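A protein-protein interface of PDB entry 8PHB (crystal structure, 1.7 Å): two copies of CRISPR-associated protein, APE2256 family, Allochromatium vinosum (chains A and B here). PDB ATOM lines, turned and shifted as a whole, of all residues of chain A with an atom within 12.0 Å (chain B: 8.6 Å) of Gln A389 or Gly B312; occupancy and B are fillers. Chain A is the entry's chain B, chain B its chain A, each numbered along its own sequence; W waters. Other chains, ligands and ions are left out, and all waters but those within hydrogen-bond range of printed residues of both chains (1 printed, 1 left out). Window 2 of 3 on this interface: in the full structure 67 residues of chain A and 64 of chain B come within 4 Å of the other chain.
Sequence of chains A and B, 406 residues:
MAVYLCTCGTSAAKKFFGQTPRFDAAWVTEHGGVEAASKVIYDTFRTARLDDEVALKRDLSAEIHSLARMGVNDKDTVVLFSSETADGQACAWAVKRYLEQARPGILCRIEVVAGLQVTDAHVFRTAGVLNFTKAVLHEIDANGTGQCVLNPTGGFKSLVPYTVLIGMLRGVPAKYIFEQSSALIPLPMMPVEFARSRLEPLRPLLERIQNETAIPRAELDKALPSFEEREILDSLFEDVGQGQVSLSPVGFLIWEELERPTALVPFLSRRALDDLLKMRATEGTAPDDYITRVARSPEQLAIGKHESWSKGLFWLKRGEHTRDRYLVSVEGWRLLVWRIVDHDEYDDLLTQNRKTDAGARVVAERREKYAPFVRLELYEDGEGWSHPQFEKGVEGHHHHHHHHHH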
ATOM      1  N   TYR A 379      12.554  -6.242 -36.736  1.00  0.00           N
ATOM      2  CA  TYR A 379      11.600  -5.451 -35.973  1.00  0.00           C
ATOM      3  C   TYR A 379      12.157  -5.342 -34.564  1.00  0.00           C
ATOM      4  O   TYR A 379      12.223  -6.347 -33.848  1.00  0.00           O
ATOM      5  CB  TYR A 379      10.218  -6.099 -35.981  1.00  0.00           C
ATOM      6  CG  TYR A 379       9.172  -5.342 -35.199  1.00  0.00           C
ATOM      7  CD1 TYR A 379       8.976  -3.980 -35.398  1.00  0.00           C
ATOM      8  CD2 TYR A 379       8.366  -5.995 -34.272  1.00  0.00           C
ATOM      9  CE1 TYR A 379       8.007  -3.287 -34.690  1.00  0.00           C
ATOM     10  CE2 TYR A 379       7.397  -5.311 -33.564  1.00  0.00           C
ATOM     11  CZ  TYR A 379       7.221  -3.958 -33.777  1.00  0.00           C
ATOM     12  OH  TYR A 379       6.256  -3.277 -33.081  1.00  0.00           O
ATOM     13  N   SER A 386       2.553   1.841 -28.844  1.00  0.00           N
ATOM     14  CA  SER A 386       1.438   2.108 -27.950  1.00  0.00           C
ATOM     15  C   SER A 386       0.096   2.071 -28.684  1.00  0.00           C
ATOM     16  O   SER A 386      -0.485   3.116 -28.986  1.00  0.00           O
ATOM     17  CB  SER A 386       1.615   3.465 -27.264  1.00  0.00           C
ATOM     18  N   HIS A 387      -0.392   0.870 -28.968  1.00  0.00           N
ATOM     19  CA  HIS A 387      -1.696   0.656 -29.578  1.00  0.00           C
ATOM     20  C   HIS A 387      -2.442  -0.422 -28.803  1.00  0.00           C
ATOM     21  O   HIS A 387      -1.827  -1.217 -28.085  1.00  0.00           O
ATOM     22  CB  HIS A 387      -1.560   0.247 -31.053  1.00  0.00           C
ATOM     23  CG  HIS A 387      -0.898   1.282 -31.913  1.00  0.00           C
ATOM     24  ND1 HIS A 387      -1.541   2.430 -32.325  1.00  0.00           N
ATOM     25  CD2 HIS A 387       0.347   1.337 -32.446  1.00  0.00           C
ATOM     26  CE1 HIS A 387      -0.721   3.148 -33.074  1.00  0.00           C
ATOM     27  NE2 HIS A 387       0.431   2.506 -33.163  1.00  0.00           N
ATOM     28  N   PRO A 388      -3.773  -0.472 -28.919  1.00  0.00           N
ATOM     29  CA  PRO A 388      -4.531  -1.503 -28.195  1.00  0.00           C
ATOM     30  C   PRO A 388      -4.095  -2.903 -28.596  1.00  0.00           C
ATOM     31  O   PRO A 388      -3.683  -3.148 -29.730  1.00  0.00           O
ATOM     32  CB  PRO A 388      -5.981  -1.230 -28.605  1.00  0.00           C
ATOM     33  CG  PRO A 388      -6.010   0.235 -28.906  1.00  0.00           C
ATOM     34  CD  PRO A 388      -4.664   0.523 -29.543  1.00  0.00           C
ATOM     35  N   GLN A 389      -4.189  -3.830 -27.642  1.00  0.00           N
ATOM     36  CA  GLN A 389      -3.780  -5.203 -27.908  1.00  0.00           C
ATOM     37  C   GLN A 389      -4.758  -5.869 -28.879  1.00  0.00           C
ATOM     38  O   GLN A 389      -5.812  -5.322 -29.220  1.00  0.00           O
ATOM     39  CB  GLN A 389      -3.696  -5.996 -26.603  1.00  0.00           C
ATOM     40  CG  GLN A 389      -5.041  -6.370 -26.032  1.00  0.00           C
ATOM     41  CD  GLN A 389      -4.942  -7.261 -24.808  1.00  0.00           C
ATOM     42  OE1 GLN A 389      -3.986  -7.178 -24.028  1.00  0.00           O
ATOM     43  NE2 GLN A 389      -5.938  -8.115 -24.628  1.00  0.00           N
ATOM     44  N   PHE A 390      -4.407  -7.074 -29.324  1.00  0.00           N
ATOM     45  CA  PHE A 390      -5.272  -7.784 -30.268  1.00  0.00           C
ATOM     46  C   PHE A 390      -6.569  -8.245 -29.605  1.00  0.00           C
ATOM     47  O   PHE A 390      -6.563  -8.733 -28.476  1.00  0.00           O
ATOM     48  CB  PHE A 390      -4.554  -8.986 -30.888  1.00  0.00           C
ATOM     49  CG  PHE A 390      -5.292  -9.588 -32.053  1.00  0.00           C
ATOM     50  CD1 PHE A 390      -5.147  -9.062 -33.330  1.00  0.00           C
ATOM     51  CD2 PHE A 390      -6.152 -10.663 -31.870  1.00  0.00           C
ATOM     52  CE1 PHE A 390      -5.828  -9.606 -34.404  1.00  0.00           C
ATOM     53  CE2 PHE A 390      -6.841 -11.209 -32.940  1.00  0.00           C
ATOM     54  CZ  PHE A 390      -6.678 -10.679 -34.208  1.00  0.00           C
ATOM     55  N   LYS B 305      -6.927 -19.058 -30.534  1.00  0.00           N
ATOM     56  CA  LYS B 305      -6.496 -18.178 -29.449  1.00  0.00           C
ATOM     57  C   LYS B 305      -7.039 -18.661 -28.110  1.00  0.00           C
ATOM     58  O   LYS B 305      -8.242 -18.853 -27.946  1.00  0.00           O
ATOM     59  CB  LYS B 305      -6.938 -16.737 -29.713  1.00  0.00           C
ATOM     60  CG  LYS B 305      -6.713 -15.804 -28.533  1.00  0.00           C
ATOM     61  CD  LYS B 305      -7.124 -14.372 -28.837  1.00  0.00           C
ATOM     62  CE  LYS B 305      -7.410 -13.585 -27.554  1.00  0.00           C
ATOM     63  NZ  LYS B 305      -6.195 -13.204 -26.782  1.00  0.00           N
ATOM     64  N   GLU B 307      -5.801 -19.141 -23.569  1.00  0.00           N
ATOM     65  CA  GLU B 307      -4.862 -18.999 -22.468  1.00  0.00           C
ATOM     66  C   GLU B 307      -4.144 -17.646 -22.498  1.00  0.00           C
ATOM     67  O   GLU B 307      -2.916 -17.549 -22.489  1.00  0.00           O
ATOM     68  CB  GLU B 307      -3.873 -20.163 -22.478  1.00  0.00           C
ATOM     69  CG  GLU B 307      -3.253 -20.421 -21.153  1.00  0.00           C
ATOM     70  CD  GLU B 307      -4.272 -20.401 -20.026  1.00  0.00           C
ATOM     71  OE1 GLU B 307      -5.269 -21.147 -20.106  1.00  0.00           O
ATOM     72  OE2 GLU B 307      -4.084 -19.605 -19.089  1.00  0.00           O
ATOM     73  N   SER B 308      -4.941 -16.588 -22.475  1.00  0.00           N
ATOM     74  CA  SER B 308      -4.384 -15.247 -22.534  1.00  0.00           C
ATOM     75  C   SER B 308      -3.480 -14.967 -21.345  1.00  0.00           C
ATOM     76  O   SER B 308      -3.817 -15.262 -20.194  1.00  0.00           O
ATOM     77  CB  SER B 308      -5.504 -14.209 -22.577  1.00  0.00           C
ATOM     78  OG  SER B 308      -6.264 -14.362 -23.759  1.00  0.00           O
ATOM     79  N   TRP B 309      -2.335 -14.375 -21.640  1.00  0.00           N
ATOM     80  CA  TRP B 309      -1.406 -13.831 -20.672  1.00  0.00           C
ATOM     81  C   TRP B 309      -1.589 -12.318 -20.649  1.00  0.00           C
ATOM     82  O   TRP B 309      -2.419 -11.764 -21.375  1.00  0.00           O
ATOM     83  CB  TRP B 309       0.033 -14.220 -21.033  1.00  0.00           C
ATOM     84  CG  TRP B 309       0.433 -15.614 -20.650  1.00  0.00           C
ATOM     85  CD1 TRP B 309      -0.392 -16.643 -20.275  1.00  0.00           C
ATOM     86  CD2 TRP B 309       1.773 -16.128 -20.588  1.00  0.00           C
ATOM     87  NE1 TRP B 309       0.360 -17.764 -19.967  1.00  0.00           N
ATOM     88  CE2 TRP B 309       1.687 -17.472 -20.150  1.00  0.00           C
ATOM     89  CE3 TRP B 309       3.035 -15.576 -20.831  1.00  0.00           C
ATOM     90  CZ2 TRP B 309       2.807 -18.277 -19.985  1.00  0.00           C
ATOM     91  CZ3 TRP B 309       4.167 -16.388 -20.661  1.00  0.00           C
ATOM     92  CH2 TRP B 309       4.042 -17.726 -20.250  1.00  0.00           C
ATOM     93  N   SER B 310      -0.802 -11.628 -19.820  1.00  0.00           N
ATOM     94  CA  SER B 310      -0.844 -10.171 -19.877  1.00  0.00           C
ATOM     95  C   SER B 310      -0.063  -9.650 -21.085  1.00  0.00           C
ATOM     96  O   SER B 310       0.596 -10.404 -21.814  1.00  0.00           O
ATOM     97  CB  SER B 310      -0.278  -9.564 -18.598  1.00  0.00           C
ATOM     98  OG  SER B 310       1.116  -9.775 -18.556  1.00  0.00           O
ATOM     99  N   LYS B 311      -0.130  -8.328 -21.289  1.00  0.00           N
ATOM    100  CA  LYS B 311       0.678  -7.620 -22.305  1.00  0.00           C
ATOM    101  C   LYS B 311       0.323  -8.033 -23.734  1.00  0.00           C
ATOM    102  O   LYS B 311       1.161  -7.935 -24.643  1.00  0.00           O
ATOM    103  CB  LYS B 311       2.187  -7.825 -22.076  1.00  0.00           C
ATOM    104  CG  LYS B 311       2.644  -7.657 -20.631  1.00  0.00           C
ATOM    105  CD  LYS B 311       2.298  -6.275 -20.093  1.00  0.00           C
ATOM    106  CE  LYS B 311       2.849  -6.096 -18.673  1.00  0.00           C
ATOM    107  NZ  LYS B 311       2.743  -4.690 -18.222  1.00  0.00           N
ATOM    108  N   GLY B 312      -0.900  -8.511 -23.946  1.00  0.00           N
ATOM    109  CA  GLY B 312      -1.339  -8.915 -25.265  1.00  0.00           C
ATOM    110  C   GLY B 312      -0.846 -10.265 -25.734  1.00  0.00           C
ATOM    111  O   GLY B 312      -1.088 -10.622 -26.891  1.00  0.00           O
ATOM    112  N   LEU B 313      -0.169 -11.020 -24.884  1.00  0.00           N
ATOM    113  CA  LEU B 313       0.365 -12.329 -25.245  1.00  0.00           C
ATOM    114  C   LEU B 313      -0.711 -13.400 -25.089  1.00  0.00           C
ATOM    115  O   LEU B 313      -1.558 -13.312 -24.202  1.00  0.00           O
ATOM    116  CB  LEU B 313       1.576 -12.664 -24.368  1.00  0.00           C
ATOM    117  CG  LEU B 313       2.812 -11.800 -24.586  1.00  0.00           C
ATOM    118  CD1 LEU B 313       3.717 -11.895 -23.350  1.00  0.00           C
ATOM    119  CD2 LEU B 313       3.560 -12.317 -25.795  1.00  0.00           C
ATOM    120  N   PHE B 314      -0.705 -14.392 -25.972  1.00  0.00           N
ATOM    121  CA  PHE B 314      -1.638 -15.508 -25.845  1.00  0.00           C
ATOM    122  C   PHE B 314      -1.077 -16.706 -26.593  1.00  0.00           C
ATOM    123  O   PHE B 314      -0.058 -16.616 -27.278  1.00  0.00           O
ATOM    124  CB  PHE B 314      -3.040 -15.148 -26.359  1.00  0.00           C
ATOM    125  CG  PHE B 314      -3.064 -14.670 -27.801  1.00  0.00           C
ATOM    126  CD1 PHE B 314      -2.806 -13.341 -28.113  1.00  0.00           C
ATOM    127  CD2 PHE B 314      -3.368 -15.555 -28.843  1.00  0.00           C
ATOM    128  CE1 PHE B 314      -2.843 -12.908 -29.448  1.00  0.00           C
ATOM    129  CE2 PHE B 314      -3.427 -15.128 -30.157  1.00  0.00           C
ATOM    130  CZ  PHE B 314      -3.161 -13.805 -30.471  1.00  0.00           C
ATOM    131  N   TRP B 315      -1.753 -17.840 -26.448  1.00  0.00           N
ATOM    132  CA  TRP B 315      -1.257 -19.106 -26.969  1.00  0.00           C
ATOM    133  C   TRP B 315      -2.107 -19.595 -28.133  1.00  0.00           C
ATOM    134  O   TRP B 315      -3.325 -19.420 -28.154  1.00  0.00           O
ATOM    135  CB  TRP B 315      -1.250 -20.184 -25.886  1.00  0.00           C
ATOM    136  CG  TRP B 315      -0.209 -19.966 -24.859  1.00  0.00           C
ATOM    137  CD1 TRP B 315      -0.349 -19.321 -23.648  1.00  0.00           C
ATOM    138  CD2 TRP B 315       1.151 -20.392 -24.936  1.00  0.00           C
ATOM    139  NE1 TRP B 315       0.856 -19.327 -22.982  1.00  0.00           N
ATOM    140  CE2 TRP B 315       1.787 -19.982 -23.749  1.00  0.00           C
ATOM    141  CE3 TRP B 315       1.899 -21.085 -25.908  1.00  0.00           C
ATOM    142  CZ2 TRP B 315       3.133 -20.237 -23.497  1.00  0.00           C
ATOM    143  CZ3 TRP B 315       3.231 -21.337 -25.659  1.00  0.00           C
ATOM    144  CH2 TRP B 315       3.839 -20.918 -24.455  1.00  0.00           C
ATOM    145  N   LEU B 327       3.529 -19.139 -28.401  1.00  0.00           N
ATOM    146  CA  LEU B 327       3.295 -17.942 -27.601  1.00  0.00           C
ATOM    147  C   LEU B 327       3.415 -16.740 -28.529  1.00  0.00           C
ATOM    148  O   LEU B 327       4.485 -16.503 -29.105  1.00  0.00           O
ATOM    149  CB  LEU B 327       4.294 -17.853 -26.450  1.00  0.00           C
ATOM    150  CG  LEU B 327       4.141 -16.619 -25.569  1.00  0.00           C
ATOM    151  CD1 LEU B 327       2.735 -16.582 -24.917  1.00  0.00           C
ATOM    152  CD2 LEU B 327       5.225 -16.625 -24.479  1.00  0.00           C
ATOM    153  N   VAL B 328       2.312 -16.008 -28.706  1.00  0.00           N
ATOM    154  CA  VAL B 328       2.232 -14.986 -29.741  1.00  0.00           C
ATOM    155  C   VAL B 328       1.629 -13.701 -29.185  1.00  0.00           C
ATOM    156  O   VAL B 328       0.987 -13.675 -28.129  1.00  0.00           O
ATOM    157  CB  VAL B 328       1.406 -15.442 -30.969  1.00  0.00           C
ATOM    158  CG1 VAL B 328       1.907 -16.787 -31.549  1.00  0.00           C
ATOM    159  CG2 VAL B 328      -0.061 -15.512 -30.624  1.00  0.00           C
ATOM    160  N   SER B 329       1.845 -12.619 -29.933  1.00  0.00           N
ATOM    161  CA  SER B 329       1.110 -11.378 -29.738  1.00  0.00           C
ATOM    162  C   SER B 329       0.992 -10.685 -31.091  1.00  0.00           C
ATOM    163  O   SER B 329       1.700 -11.019 -32.049  1.00  0.00           O
ATOM    164  CB  SER B 329       1.778 -10.453 -28.716  1.00  0.00           C
ATOM    165  OG  SER B 329       3.001  -9.942 -29.207  1.00  0.00           O
ATOM    166  N   VAL B 330       0.102  -9.699 -31.167  1.00  0.00           N
ATOM    167  CA  VAL B 330      -0.124  -8.975 -32.415  1.00  0.00           C
ATOM    168  C   VAL B 330       0.224  -7.515 -32.194  1.00  0.00           C
ATOM    169  O   VAL B 330      -0.290  -6.886 -31.267  1.00  0.00           O
ATOM    170  CB  VAL B 330      -1.569  -9.132 -32.914  1.00  0.00           C
ATOM    171  CG1 VAL B 330      -1.790  -8.281 -34.186  1.00  0.00           C
ATOM    172  CG2 VAL B 330      -1.857 -10.588 -33.193  1.00  0.00           C
ATOM    173  N   GLU B 331       1.111  -6.984 -33.027  1.00  0.00           N
ATOM    174  CA  GLU B 331       1.446  -5.562 -33.002  1.00  0.00           C
ATOM    175  C   GLU B 331       1.226  -5.019 -34.404  1.00  0.00           C
ATOM    176  O   GLU B 331       2.039  -5.256 -35.305  1.00  0.00           O
ATOM    177  CB  GLU B 331       2.867  -5.314 -32.524  1.00  0.00           C
ATOM    178  CG  GLU B 331       3.010  -5.520 -31.029  1.00  0.00           C
ATOM    179  CD  GLU B 331       4.444  -5.358 -30.529  1.00  0.00           C
ATOM    180  OE1 GLU B 331       5.324  -4.890 -31.285  1.00  0.00           O
ATOM    181  OE2 GLU B 331       4.690  -5.697 -29.366  1.00  0.00           O
ATOM    182  N   GLY B 332       0.125  -4.295 -34.570  1.00  0.00           N
ATOM    183  CA  GLY B 332      -0.205  -3.763 -35.880  1.00  0.00           C
ATOM    184  C   GLY B 332      -0.407  -4.904 -36.853  1.00  0.00           C
ATOM    185  O   GLY B 332      -1.257  -5.779 -36.654  1.00  0.00           O
ATOM    186  N   LEU B 335       2.308 -10.465 -36.664  1.00  0.00           N
ATOM    187  CA  LEU B 335       2.051 -11.534 -35.709  1.00  0.00           C
ATOM    188  C   LEU B 335       3.391 -11.954 -35.126  1.00  0.00           C
ATOM    189  O   LEU B 335       4.197 -12.587 -35.813  1.00  0.00           O
ATOM    190  CB  LEU B 335       1.340 -12.706 -36.377  1.00  0.00           C
ATOM    191  CG  LEU B 335       1.059 -13.953 -35.529  1.00  0.00           C
ATOM    192  CD1 LEU B 335       0.107 -13.652 -34.374  1.00  0.00           C
ATOM    193  CD2 LEU B 335       0.506 -15.053 -36.428  1.00  0.00           C
ATOM    194  N   LEU B 336       3.637 -11.585 -33.864  1.00  0.00           N
ATOM    195  CA  LEU B 336       4.913 -11.844 -33.205  1.00  0.00           C
ATOM    196  C   LEU B 336       4.875 -13.227 -32.571  1.00  0.00           C
ATOM    197  O   LEU B 336       4.006 -13.509 -31.741  1.00  0.00           O
ATOM    198  CB  LEU B 336       5.216 -10.782 -32.145  1.00  0.00           C
ATOM    199  CG  LEU B 336       5.210  -9.329 -32.639  1.00  0.00           C
ATOM    200  CD1 LEU B 336       5.774  -8.439 -31.540  1.00  0.00           C
ATOM    201  CD2 LEU B 336       6.036  -9.191 -33.902  1.00  0.00           C
ATOM    202  N   TRP B 338       6.757 -15.405 -30.096  1.00  0.00           N
ATOM    203  CA  TRP B 338       7.757 -15.278 -29.037  1.00  0.00           C
ATOM    204  C   TRP B 338       8.459 -16.605 -28.764  1.00  0.00           C
ATOM    205  O   TRP B 338       9.684 -16.640 -28.631  1.00  0.00           O
ATOM    206  CB  TRP B 338       7.099 -14.734 -27.753  1.00  0.00           C
ATOM    207  CG  TRP B 338       6.572 -13.321 -27.924  1.00  0.00           C
ATOM    208  CD1 TRP B 338       5.465 -12.938 -28.629  1.00  0.00           C
ATOM    209  CD2 TRP B 338       7.135 -12.118 -27.381  1.00  0.00           C
ATOM    210  NE1 TRP B 338       5.319 -11.576 -28.573  1.00  0.00           N
ATOM    211  CE2 TRP B 338       6.326 -11.048 -27.808  1.00  0.00           C
ATOM    212  CE3 TRP B 338       8.249 -11.842 -26.589  1.00  0.00           C
ATOM    213  CZ2 TRP B 338       6.594  -9.720 -27.460  1.00  0.00           C
ATOM    214  CZ3 TRP B 338       8.514 -10.531 -26.235  1.00  0.00           C
ATOM    215  CH2 TRP B 338       7.690  -9.483 -26.668  1.00  0.00           C
ATOM    216  N   ASP B 357       3.082 -12.786 -12.814  1.00  0.00           N
ATOM    217  CA  ASP B 357       2.579 -12.197 -14.058  1.00  0.00           C
ATOM    218  C   ASP B 357       3.617 -12.534 -15.122  1.00  0.00           C
ATOM    219  O   ASP B 357       4.564 -11.785 -15.369  1.00  0.00           O
ATOM    220  CB  ASP B 357       2.373 -10.700 -13.910  1.00  0.00           C
ATOM    221  CG  ASP B 357       1.627 -10.104 -15.088  1.00  0.00           C
ATOM    222  OD1 ASP B 357       1.673 -10.726 -16.155  1.00  0.00           O
ATOM    223  OD2 ASP B 357       0.986  -9.042 -14.939  1.00  0.00           O
ATOM    224  N   GLY B 359       3.463 -12.791 -18.408  1.00  0.00           N
ATOM    225  CA  GLY B 359       3.534 -11.913 -19.571  1.00  0.00           C
ATOM    226  C   GLY B 359       4.369 -10.672 -19.315  1.00  0.00           C
ATOM    227  O   GLY B 359       5.146 -10.248 -20.171  1.00  0.00           O
ATOM    228  N   ALA B 360       4.209 -10.064 -18.140  1.00  0.00           N
ATOM    229  CA  ALA B 360       5.032  -8.915 -17.780  1.00  0.00           C
ATOM    230  C   ALA B 360       6.510  -9.282 -17.745  1.00  0.00           C
ATOM    231  O   ALA B 360       7.369  -8.492 -18.156  1.00  0.00           O
ATOM    232  CB  ALA B 360       4.581  -8.367 -16.423  1.00  0.00           C
ATOM    233  N   VAL B 363       7.851  -9.527 -21.430  1.00  0.00           N
ATOM    234  CA  VAL B 363       8.057  -8.253 -22.110  1.00  0.00           C
ATOM    235  C   VAL B 363       9.251  -7.506 -21.529  1.00  0.00           C
ATOM    236  O   VAL B 363       9.954  -6.782 -22.248  1.00  0.00           O
ATOM    237  CB  VAL B 363       6.748  -7.439 -22.050  1.00  0.00           C
ATOM    238  CG1 VAL B 363       6.955  -6.001 -22.510  1.00  0.00           C
ATOM    239  CG2 VAL B 363       5.712  -8.120 -22.921  1.00  0.00           C
HETATM  240  O   HOH W   1      -1.887  -9.385 -29.018  1.00  0.00           O
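Printed residues of chain A that touch a printed residue of chain B: Tyr A379, Gln A389 and Phe A390. Hydrophobic or aromatic side chains of chain B within 4 Å of the printed part of chain A: Val B330 and Leu B336. Among the printed residues, no Asp or Glu carboxylate lies within 4 Å of a Lys or Arg side-chain nitrogen of the other chain.
N of Gly B312 lies within hydrogen-bond range of OE1 of Gln A389, at 3.4 Å. The side-chain carboxylate (OE1) of Glu B331 sits at hydrogen-bond distance from the side-chain hydroxyl (OH) of Tyr A379, 2.6 Å away.
Tyr A379 touches Leu B336. Phe A390 touches Val B330 (CD1 to CG1, 3.6 Å).
His A387 touches none of the printed residues of chain B. Gln A389 touches just one residue of chain B: Gly B312. Printed residues of chain B within 4 Å of Phe A390: Val B330 (3.6 Å). No residue of chain A comes within 4 Å of Ser B310. No residue of chain A comes within 4 Å of Lys B311. No residue of chain A comes within 4 Å of Phe B314. Val B330 touches just one residue of chain A: Phe A390. Printed residues of chain A within 4 Å of Leu B336: Tyr A379 (3.97 Å). The nearest residue of chain B that does not touch Gln A389 is Lys B311 (4.4 Å). The nearest residue of chain A that does not touch Gly B312 is Phe A390 (5.4 Å). The nearest printed residue of chain B that does not touch Phe A390 is Phe B314 (4.5 Å).
Water W1 lies within hydrogen-bond range of O of Gly B312 (2.6 Å), N of Val B330 (2.9 Å) and N of Phe A390 (3.4 Å).
N of Leu B336 is in hydrogen-bond range of O of Ser B329 (2.7 Å).
No position is printed for both chains. Of the 4 pairs that touch across the chains among the printed residues, none has its exchanged pair printed and touching as well.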
